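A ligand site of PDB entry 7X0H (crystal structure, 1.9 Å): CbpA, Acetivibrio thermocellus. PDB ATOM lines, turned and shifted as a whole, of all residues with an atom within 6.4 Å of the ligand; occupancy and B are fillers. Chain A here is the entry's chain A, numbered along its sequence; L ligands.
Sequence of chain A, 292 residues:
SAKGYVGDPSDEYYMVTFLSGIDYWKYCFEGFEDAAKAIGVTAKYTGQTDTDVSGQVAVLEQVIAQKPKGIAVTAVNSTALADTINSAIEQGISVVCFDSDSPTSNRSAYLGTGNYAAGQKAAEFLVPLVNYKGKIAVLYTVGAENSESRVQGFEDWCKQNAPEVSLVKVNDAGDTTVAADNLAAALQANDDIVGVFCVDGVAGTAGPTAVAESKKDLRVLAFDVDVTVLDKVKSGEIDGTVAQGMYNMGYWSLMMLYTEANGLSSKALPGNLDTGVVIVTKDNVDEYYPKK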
ATOM      1  N   PHE A  18      -1.678  22.945 -20.860  1.00  0.00           N
ATOM      2  CA  PHE A  18      -1.559  24.367 -21.130  1.00  0.00           C
ATOM      3  C   PHE A  18      -1.844  24.566 -22.609  1.00  0.00           C
ATOM      4  O   PHE A  18      -1.903  23.601 -23.377  1.00  0.00           O
ATOM      5  CB  PHE A  18      -0.178  24.914 -20.732  1.00  0.00           C
ATOM      6  CG  PHE A  18       0.978  24.267 -21.438  1.00  0.00           C
ATOM      7  CD1 PHE A  18       1.552  23.109 -20.935  1.00  0.00           C
ATOM      8  CD2 PHE A  18       1.532  24.844 -22.573  1.00  0.00           C
ATOM      9  CE1 PHE A  18       2.626  22.513 -21.574  1.00  0.00           C
ATOM     10  CE2 PHE A  18       2.615  24.243 -23.213  1.00  0.00           C
ATOM     11  CZ  PHE A  18       3.154  23.082 -22.708  1.00  0.00           C
ATOM     12  N   LEU A  19      -2.050  25.813 -23.024  1.00  0.00           N
ATOM     13  CA  LEU A  19      -2.574  26.096 -24.356  1.00  0.00           C
ATOM     14  C   LEU A  19      -3.743  25.155 -24.658  1.00  0.00           C
ATOM     15  O   LEU A  19      -3.807  24.483 -25.679  1.00  0.00           O
ATOM     16  CB  LEU A  19      -1.471  25.972 -25.410  1.00  0.00           C
ATOM     17  CG  LEU A  19      -0.342  27.012 -25.401  1.00  0.00           C
ATOM     18  CD1 LEU A  19       0.859  26.582 -26.227  1.00  0.00           C
ATOM     19  CD2 LEU A  19      -0.879  28.352 -25.905  1.00  0.00           C
ATOM     20  N   ILE A  22      -5.981  24.009 -28.041  1.00  0.00           N
ATOM     21  CA  ILE A  22      -5.475  23.685 -29.369  1.00  0.00           C
ATOM     22  C   ILE A  22      -5.763  22.225 -29.704  1.00  0.00           C
ATOM     23  O   ILE A  22      -5.983  21.373 -28.823  1.00  0.00           O
ATOM     24  CB  ILE A  22      -3.970  23.985 -29.513  1.00  0.00           C
ATOM     25  CG1 ILE A  22      -3.143  23.121 -28.562  1.00  0.00           C
ATOM     26  CG2 ILE A  22      -3.686  25.473 -29.265  1.00  0.00           C
ATOM     27  CD1 ILE A  22      -1.639  23.332 -28.702  1.00  0.00           C
ATOM     28  N   TYR A  24      -3.943  19.865 -30.728  1.00  0.00           N
ATOM     29  CA  TYR A  24      -2.957  18.880 -30.263  1.00  0.00           C
ATOM     30  C   TYR A  24      -3.499  18.058 -29.094  1.00  0.00           C
ATOM     31  O   TYR A  24      -3.360  16.828 -29.075  1.00  0.00           O
ATOM     32  CB  TYR A  24      -1.665  19.608 -29.870  1.00  0.00           C
ATOM     33  CG  TYR A  24      -0.560  18.718 -29.375  1.00  0.00           C
ATOM     34  CD1 TYR A  24       0.283  18.058 -30.248  1.00  0.00           C
ATOM     35  CD2 TYR A  24      -0.339  18.566 -28.011  1.00  0.00           C
ATOM     36  CE1 TYR A  24       1.292  17.253 -29.794  1.00  0.00           C
ATOM     37  CE2 TYR A  24       0.671  17.761 -27.547  1.00  0.00           C
ATOM     38  CZ  TYR A  24       1.477  17.097 -28.438  1.00  0.00           C
ATOM     39  OH  TYR A  24       2.487  16.292 -27.984  1.00  0.00           O
ATOM     40  N   TRP A  25      -4.149  18.706 -28.120  1.00  0.00           N
ATOM     41  CA  TRP A  25      -4.631  17.978 -26.948  1.00  0.00           C
ATOM     42  C   TRP A  25      -5.844  17.105 -27.254  1.00  0.00           C
ATOM     43  O   TRP A  25      -6.124  16.175 -26.494  1.00  0.00           O
ATOM     44  CB  TRP A  25      -4.975  18.957 -25.809  1.00  0.00           C
ATOM     45  CG  TRP A  25      -3.879  19.936 -25.541  1.00  0.00           C
ATOM     46  CD1 TRP A  25      -3.942  21.291 -25.696  1.00  0.00           C
ATOM     47  CD2 TRP A  25      -2.545  19.641 -25.121  1.00  0.00           C
ATOM     48  NE1 TRP A  25      -2.740  21.854 -25.389  1.00  0.00           N
ATOM     49  CE2 TRP A  25      -1.854  20.868 -25.030  1.00  0.00           C
ATOM     50  CE3 TRP A  25      -1.858  18.466 -24.795  1.00  0.00           C
ATOM     51  CZ2 TRP A  25      -0.517  20.954 -24.627  1.00  0.00           C
ATOM     52  CZ3 TRP A  25      -0.535  18.548 -24.402  1.00  0.00           C
ATOM     53  CH2 TRP A  25       0.114  19.786 -24.327  1.00  0.00           C
ATOM     54  N   THR A  74       0.898  17.879 -18.182  1.00  0.00           N
ATOM     55  CA  THR A  74       2.002  18.398 -18.966  1.00  0.00           C
ATOM     56  C   THR A  74       2.335  19.782 -18.426  1.00  0.00           C
ATOM     57  O   THR A  74       1.471  20.663 -18.391  1.00  0.00           O
ATOM     58  CB  THR A  74       1.661  18.447 -20.461  1.00  0.00           C
ATOM     59  OG1 THR A  74       2.738  19.077 -21.157  1.00  0.00           O
ATOM     60  CG2 THR A  74       0.364  19.191 -20.735  1.00  0.00           C
ATOM     61  N   ASP A  99       3.961  14.493 -22.196  1.00  0.00           N
ATOM     62  CA  ASP A  99       4.239  15.522 -23.190  1.00  0.00           C
ATOM     63  C   ASP A  99       5.354  16.476 -22.804  1.00  0.00           C
ATOM     64  O   ASP A  99       6.276  16.684 -23.598  1.00  0.00           O
ATOM     65  CB  ASP A  99       2.955  16.317 -23.501  1.00  0.00           C
ATOM     66  CG  ASP A  99       3.217  17.520 -24.404  1.00  0.00           C
ATOM     67  OD1 ASP A  99       3.506  17.324 -25.603  1.00  0.00           O
ATOM     68  OD2 ASP A  99       3.157  18.646 -23.891  1.00  0.00           O
ATOM     69  N   SER A 100       5.282  17.100 -21.630  1.00  0.00           N
ATOM     70  CA  SER A 100       6.343  17.977 -21.136  1.00  0.00           C
ATOM     71  C   SER A 100       6.525  17.707 -19.656  1.00  0.00           C
ATOM     72  O   SER A 100       5.579  17.827 -18.872  1.00  0.00           O
ATOM     73  CB  SER A 100       6.022  19.456 -21.381  1.00  0.00           C
ATOM     74  OG  SER A 100       7.190  20.246 -21.249  1.00  0.00           O
ATOM     75  N   THR A 113       7.335  12.210 -25.998  1.00  0.00           N
ATOM     76  CA  THR A 113       8.468  12.234 -26.913  1.00  0.00           C
ATOM     77  C   THR A 113       9.764  12.226 -26.133  1.00  0.00           C
ATOM     78  O   THR A 113       9.858  12.791 -25.030  1.00  0.00           O
ATOM     79  CB  THR A 113       8.360  13.481 -27.795  1.00  0.00           C
ATOM     80  OG1 THR A 113       7.174  13.377 -28.597  1.00  0.00           O
ATOM     81  CG2 THR A 113       9.577  13.663 -28.675  1.00  0.00           C
ATOM     82  N   ASN A 115      12.489  14.062 -26.032  1.00  0.00           N
ATOM     83  CA  ASN A 115      12.584  15.396 -26.617  1.00  0.00           C
ATOM     84  C   ASN A 115      14.018  15.731 -27.027  1.00  0.00           C
ATOM     85  O   ASN A 115      14.218  16.330 -28.083  1.00  0.00           O
ATOM     86  CB  ASN A 115      12.018  16.404 -25.626  1.00  0.00           C
ATOM     87  CG  ASN A 115      10.514  16.284 -25.501  1.00  0.00           C
ATOM     88  OD1 ASN A 115       9.775  16.485 -26.466  1.00  0.00           O
ATOM     89  ND2 ASN A 115      10.050  15.917 -24.308  1.00  0.00           N
ATOM     90  N   THR A 141       9.110  27.539 -27.166  1.00  0.00           N
ATOM     91  CA  THR A 141       8.497  28.046 -25.942  1.00  0.00           C
ATOM     92  C   THR A 141       9.523  27.984 -24.812  1.00  0.00           C
ATOM     93  O   THR A 141       9.732  26.932 -24.194  1.00  0.00           O
ATOM     94  CB  THR A 141       7.254  27.254 -25.580  1.00  0.00           C
ATOM     95  OG1 THR A 141       6.388  27.167 -26.717  1.00  0.00           O
ATOM     96  CG2 THR A 141       6.502  27.913 -24.410  1.00  0.00           C
ATOM     97  N   ALA A 144       9.485  25.620 -21.122  1.00  0.00           N
ATOM     98  CA  ALA A 144       8.876  24.303 -21.163  1.00  0.00           C
ATOM     99  C   ALA A 144       9.955  23.249 -21.349  1.00  0.00           C
ATOM    100  O   ALA A 144      10.818  23.377 -22.226  1.00  0.00           O
ATOM    101  CB  ALA A 144       7.845  24.244 -22.291  1.00  0.00           C
ATOM    102  N   ASN A 146       9.934  20.245 -22.564  1.00  0.00           N
ATOM    103  CA  ASN A 146      10.054  19.531 -23.837  1.00  0.00           C
ATOM    104  C   ASN A 146      10.727  20.416 -24.889  1.00  0.00           C
ATOM    105  O   ASN A 146      11.648  19.967 -25.572  1.00  0.00           O
ATOM    106  CB  ASN A 146       8.691  18.989 -24.326  1.00  0.00           C
ATOM    107  CG  ASN A 146       7.589  20.021 -24.431  1.00  0.00           C
ATOM    108  OD1 ASN A 146       7.761  21.230 -24.226  1.00  0.00           O
ATOM    109  ND2 ASN A 146       6.408  19.527 -24.776  1.00  0.00           N
ATOM    110  N   SER A 147      10.321  21.685 -24.983  1.00  0.00           N
ATOM    111  CA  SER A 147      10.949  22.579 -25.951  1.00  0.00           C
ATOM    112  C   SER A 147      12.421  22.812 -25.637  1.00  0.00           C
ATOM    113  O   SER A 147      13.264  22.772 -26.542  1.00  0.00           O
ATOM    114  CB  SER A 147      10.192  23.903 -25.995  1.00  0.00           C
ATOM    115  OG  SER A 147       8.858  23.693 -26.415  1.00  0.00           O
ATOM    116  N   ARG A 150      14.355  19.752 -26.678  1.00  0.00           N
ATOM    117  CA  ARG A 150      14.490  19.668 -28.124  1.00  0.00           C
ATOM    118  C   ARG A 150      15.572  20.625 -28.609  1.00  0.00           C
ATOM    119  O   ARG A 150      16.392  20.269 -29.463  1.00  0.00           O
ATOM    120  CB  ARG A 150      13.157  19.984 -28.813  1.00  0.00           C
ATOM    121  CG  ARG A 150      12.089  18.939 -28.585  1.00  0.00           C
ATOM    122  CD  ARG A 150      10.697  19.389 -29.022  1.00  0.00           C
ATOM    123  NE  ARG A 150       9.677  18.551 -28.392  1.00  0.00           N
ATOM    124  CZ  ARG A 150       8.360  18.758 -28.447  1.00  0.00           C
ATOM    125  NH1 ARG A 150       7.870  19.798 -29.112  1.00  0.00           N
ATOM    126  NH2 ARG A 150       7.545  17.928 -27.826  1.00  0.00           N
ATOM    127  N   ASP A 172       9.130  31.748 -28.767  1.00  0.00           N
ATOM    128  CA  ASP A 172       7.788  31.874 -29.326  1.00  0.00           C
ATOM    129  C   ASP A 172       6.759  32.274 -28.270  1.00  0.00           C
ATOM    130  O   ASP A 172       5.639  32.648 -28.614  1.00  0.00           O
ATOM    131  CB  ASP A 172       7.385  30.590 -30.107  1.00  0.00           C
ATOM    132  CG  ASP A 172       7.059  29.376 -29.233  1.00  0.00           C
ATOM    133  OD1 ASP A 172       6.533  29.471 -28.108  1.00  0.00           O
ATOM    134  OD2 ASP A 172       7.311  28.253 -29.745  1.00  0.00           O
ATOM    135  N   GLY A 174       4.817  30.998 -26.358  1.00  0.00           N
ATOM    136  CA  GLY A 174       3.510  30.375 -26.324  1.00  0.00           C
ATOM    137  C   GLY A 174       2.405  31.158 -26.995  1.00  0.00           C
ATOM    138  O   GLY A 174       1.234  30.895 -26.724  1.00  0.00           O
ATOM    139  N   VAL A 199      10.054  24.384 -32.980  1.00  0.00           N
ATOM    140  CA  VAL A 199      10.278  23.344 -31.971  1.00  0.00           C
ATOM    141  C   VAL A 199       8.995  22.790 -31.381  1.00  0.00           C
ATOM    142  O   VAL A 199       9.009  21.693 -30.807  1.00  0.00           O
ATOM    143  CB  VAL A 199      11.187  23.940 -30.885  1.00  0.00           C
ATOM    144  CG1 VAL A 199      11.387  22.985 -29.729  1.00  0.00           C
ATOM    145  CG2 VAL A 199      12.518  24.369 -31.485  1.00  0.00           C
ATOM    146  N   ASP A 200       7.888  23.509 -31.515  1.00  0.00           N
ATOM    147  CA  ASP A 200       6.624  23.102 -30.918  1.00  0.00           C
ATOM    148  C   ASP A 200       5.499  23.678 -31.781  1.00  0.00           C
ATOM    149  O   ASP A 200       5.745  24.397 -32.752  1.00  0.00           O
ATOM    150  CB  ASP A 200       6.542  23.553 -29.462  1.00  0.00           C
ATOM    151  CG  ASP A 200       7.025  24.974 -29.258  1.00  0.00           C
ATOM    152  OD1 ASP A 200       6.418  25.881 -29.846  1.00  0.00           O
ATOM    153  OD2 ASP A 200       8.012  25.159 -28.512  1.00  0.00           O
ATOM    154  N   GLY A 201       4.261  23.356 -31.401  1.00  0.00           N
ATOM    155  CA  GLY A 201       3.129  23.653 -32.261  1.00  0.00           C
ATOM    156  C   GLY A 201       2.903  25.139 -32.481  1.00  0.00           C
ATOM    157  O   GLY A 201       2.526  25.563 -33.580  1.00  0.00           O
ATOM    158  N   VAL A 202       3.117  25.947 -31.439  1.00  0.00           N
ATOM    159  CA  VAL A 202       3.014  27.401 -31.596  1.00  0.00           C
ATOM    160  C   VAL A 202       3.960  27.877 -32.686  1.00  0.00           C
ATOM    161  O   VAL A 202       3.588  28.673 -33.562  1.00  0.00           O
ATOM    162  CB  VAL A 202       3.305  28.115 -30.263  1.00  0.00           C
ATOM    163  CG1 VAL A 202       3.547  29.619 -30.514  1.00  0.00           C
ATOM    164  CG2 VAL A 202       2.163  27.890 -29.289  1.00  0.00           C
ATOM    165  N   ALA A 203       5.207  27.403 -32.644  1.00  0.00           N
ATOM    166  CA  ALA A 203       6.211  27.800 -33.621  1.00  0.00           C
ATOM    167  C   ALA A 203       5.902  27.232 -34.995  1.00  0.00           C
ATOM    168  O   ALA A 203       6.261  27.849 -36.007  1.00  0.00           O
ATOM    169  CB  ALA A 203       7.586  27.334 -33.144  1.00  0.00           C
ATOM    170  N   PHE A 223       6.718  21.575 -36.371  1.00  0.00           N
ATOM    171  CA  PHE A 223       6.405  20.541 -35.356  1.00  0.00           C
ATOM    172  C   PHE A 223       4.876  20.326 -35.366  1.00  0.00           C
ATOM    173  O   PHE A 223       4.155  21.214 -35.698  1.00  0.00           O
ATOM    174  CB  PHE A 223       6.897  20.867 -33.955  1.00  0.00           C
ATOM    175  CG  PHE A 223       7.730  19.797 -33.298  1.00  0.00           C
ATOM    176  CD1 PHE A 223       9.084  19.706 -33.529  1.00  0.00           C
ATOM    177  CD2 PHE A 223       7.150  18.861 -32.455  1.00  0.00           C
ATOM    178  CE1 PHE A 223       9.851  18.717 -32.954  1.00  0.00           C
ATOM    179  CE2 PHE A 223       7.922  17.880 -31.869  1.00  0.00           C
ATOM    180  CZ  PHE A 223       9.261  17.808 -32.119  1.00  0.00           C
ATOM    181  N   ASP A 224       4.450  19.086 -35.160  1.00  0.00           N
ATOM    182  CA  ASP A 224       3.038  18.660 -35.028  1.00  0.00           C
ATOM    183  C   ASP A 224       2.309  18.656 -36.397  1.00  0.00           C
ATOM    184  O   ASP A 224       2.885  18.880 -37.394  1.00  0.00           O
ATOM    185  CB  ASP A 224       2.412  19.365 -33.831  1.00  0.00           C
ATOM    186  CG  ASP A 224       3.262  19.144 -32.622  1.00  0.00           C
ATOM    187  OD1 ASP A 224       3.626  18.015 -32.397  1.00  0.00           O
ATOM    188  OD2 ASP A 224       3.499  20.078 -31.965  1.00  0.00           O
ATOM    189  N   GLN A 244       4.172  13.559 -33.286  1.00  0.00           N
ATOM    190  CA  GLN A 244       4.323  12.907 -31.999  1.00  0.00           C
ATOM    191  C   GLN A 244       3.214  11.871 -31.788  1.00  0.00           C
ATOM    192  O   GLN A 244       2.150  11.934 -32.405  1.00  0.00           O
ATOM    193  CB  GLN A 244       4.283  13.932 -30.872  1.00  0.00           C
ATOM    194  CG  GLN A 244       5.304  15.042 -30.973  1.00  0.00           C
ATOM    195  CD  GLN A 244       5.273  15.936 -29.744  1.00  0.00           C
ATOM    196  OE1 GLN A 244       5.680  15.530 -28.655  1.00  0.00           O
ATOM    197  NE2 GLN A 244       4.782  17.162 -29.917  1.00  0.00           N
ATOM    198  N   MET A 249       0.408   8.829 -25.680  1.00  0.00           N
ATOM    199  CA  MET A 249       0.649   9.549 -24.434  1.00  0.00           C
ATOM    200  C   MET A 249      -0.560   9.485 -23.518  1.00  0.00           C
ATOM    201  O   MET A 249      -0.446   9.236 -22.315  1.00  0.00           O
ATOM    202  CB  MET A 249       0.988  11.004 -24.713  1.00  0.00           C
ATOM    203  CG  MET A 249       2.296  11.246 -25.403  1.00  0.00           C
ATOM    204  SD  MET A 249       2.539  13.029 -25.587  1.00  0.00           S
ATOM    205  CE  MET A 249       3.380  13.025 -27.172  1.00  0.00           C
HETATM  206  C1  LIG L   1       4.416  20.301 -27.502  1.00  0.00           C
HETATM  207  C2  LIG L   1       3.383  20.774 -26.531  1.00  0.00           C
HETATM  208  C3  LIG L   1       2.998  22.218 -26.785  1.00  0.00           C
HETATM  209  C4  LIG L   1       2.434  22.390 -28.192  1.00  0.00           C
HETATM  210  C5  LIG L   1       2.064  23.799 -28.600  1.00  0.00           C
HETATM  211  C6  LIG L   1       3.931  20.477 -28.932  1.00  0.00           C
HETATM  212  O1  LIG L   1       4.918  20.263 -29.865  1.00  0.00           O
HETATM  213  O2  LIG L   1       4.741  18.892 -27.382  1.00  0.00           O
HETATM  214  O3  LIG L   1       3.917  20.642 -25.190  1.00  0.00           O
HETATM  215  O4  LIG L   1       1.953  22.609 -25.869  1.00  0.00           O
HETATM  216  O5  LIG L   1       3.425  21.883 -29.183  1.00  0.00           O
HETATM  217  O6  LIG L   1       3.183  24.578 -28.737  1.00  0.00           O
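CE2 of Phe 18 touches O4 of the ligand (3.2 Å).
CD1 of Leu 19 touches C5 of the ligand, at 3.9 Å.
CD1 of Ile 22 touches C5 of the ligand, at 3.7 Å.
Trp 25 touches the ligand (CZ2 to O4, 3.2 Å).
Asp 200 touches the ligand (CA to O1, 3.5 Å).
CD2 of Phe 223 touches O1 of the ligand, at 3.7 Å.
Hydrophobic or aromatic side chains that line the ligand: Phe 18, Leu 19, Ile 22, Tyr 24, Trp 25, Val 202 and Phe 223.
The nearest printed residue that does not touch the ligand is Val 199 (4.4 Å).
OH of Tyr 24 sits at hydrogen-bond distance from OD1 of Asp 99, 2.8 Å away.
NE1 of Trp 25 lies within hydrogen-bond range of O of Phe 18, at 2.8 Å.
The backbone NH (N) of Gly 201 lies within hydrogen-bond range of the side-chain carboxylate (OD2) of Asp 224, at 3.4 Å.
OG1 of Thr 74 sits at hydrogen-bond distance from OD2 of Asp 99, at 2.8 Å.
NH1 of Arg 150 lies within hydrogen-bond range of O of Val 199 (2.8 Å).
OD1 of Asp 200 lies close to OD2 of Asp 172 (2.5 Å).
The side-chain amide nitrogen of Gln 244 lies within hydrogen-bond range of the side-chain carboxylate of Asp 224.
N of Asn 146 sits at hydrogen-bond distance from OG of Ser 100 (3.0 Å).
O5 of the ligand sits at hydrogen-bond distance from N of Gly 201 (2.8 Å).
NE2 of Gln 244 lies within hydrogen-bond range of O2 of the ligand.
OH of Tyr 24 lies within hydrogen-bond range of O2 of the ligand (3.5 Å).
An oxygen (O2) of the ligand sits at hydrogen-bond distance from the guanidinium group of Arg 150 (3.0 Å).
The side-chain carboxylate (OD2) of Asp 99 is in hydrogen-bond range of an oxygen (O3) of the ligand (2.5 Å).
The side-chain amide nitrogen (ND2) of Asn 146 sits at hydrogen-bond distance from an oxygen (O3) of the ligand, 2.8 Å away.
The side-chain carboxylate (OD2) of Asp 224 is in hydrogen-bond range of an oxygen (O1) of the ligand, 2.5 Å away.
N of Val 202 is in hydrogen-bond range of O6 of the ligand (3.0 Å).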
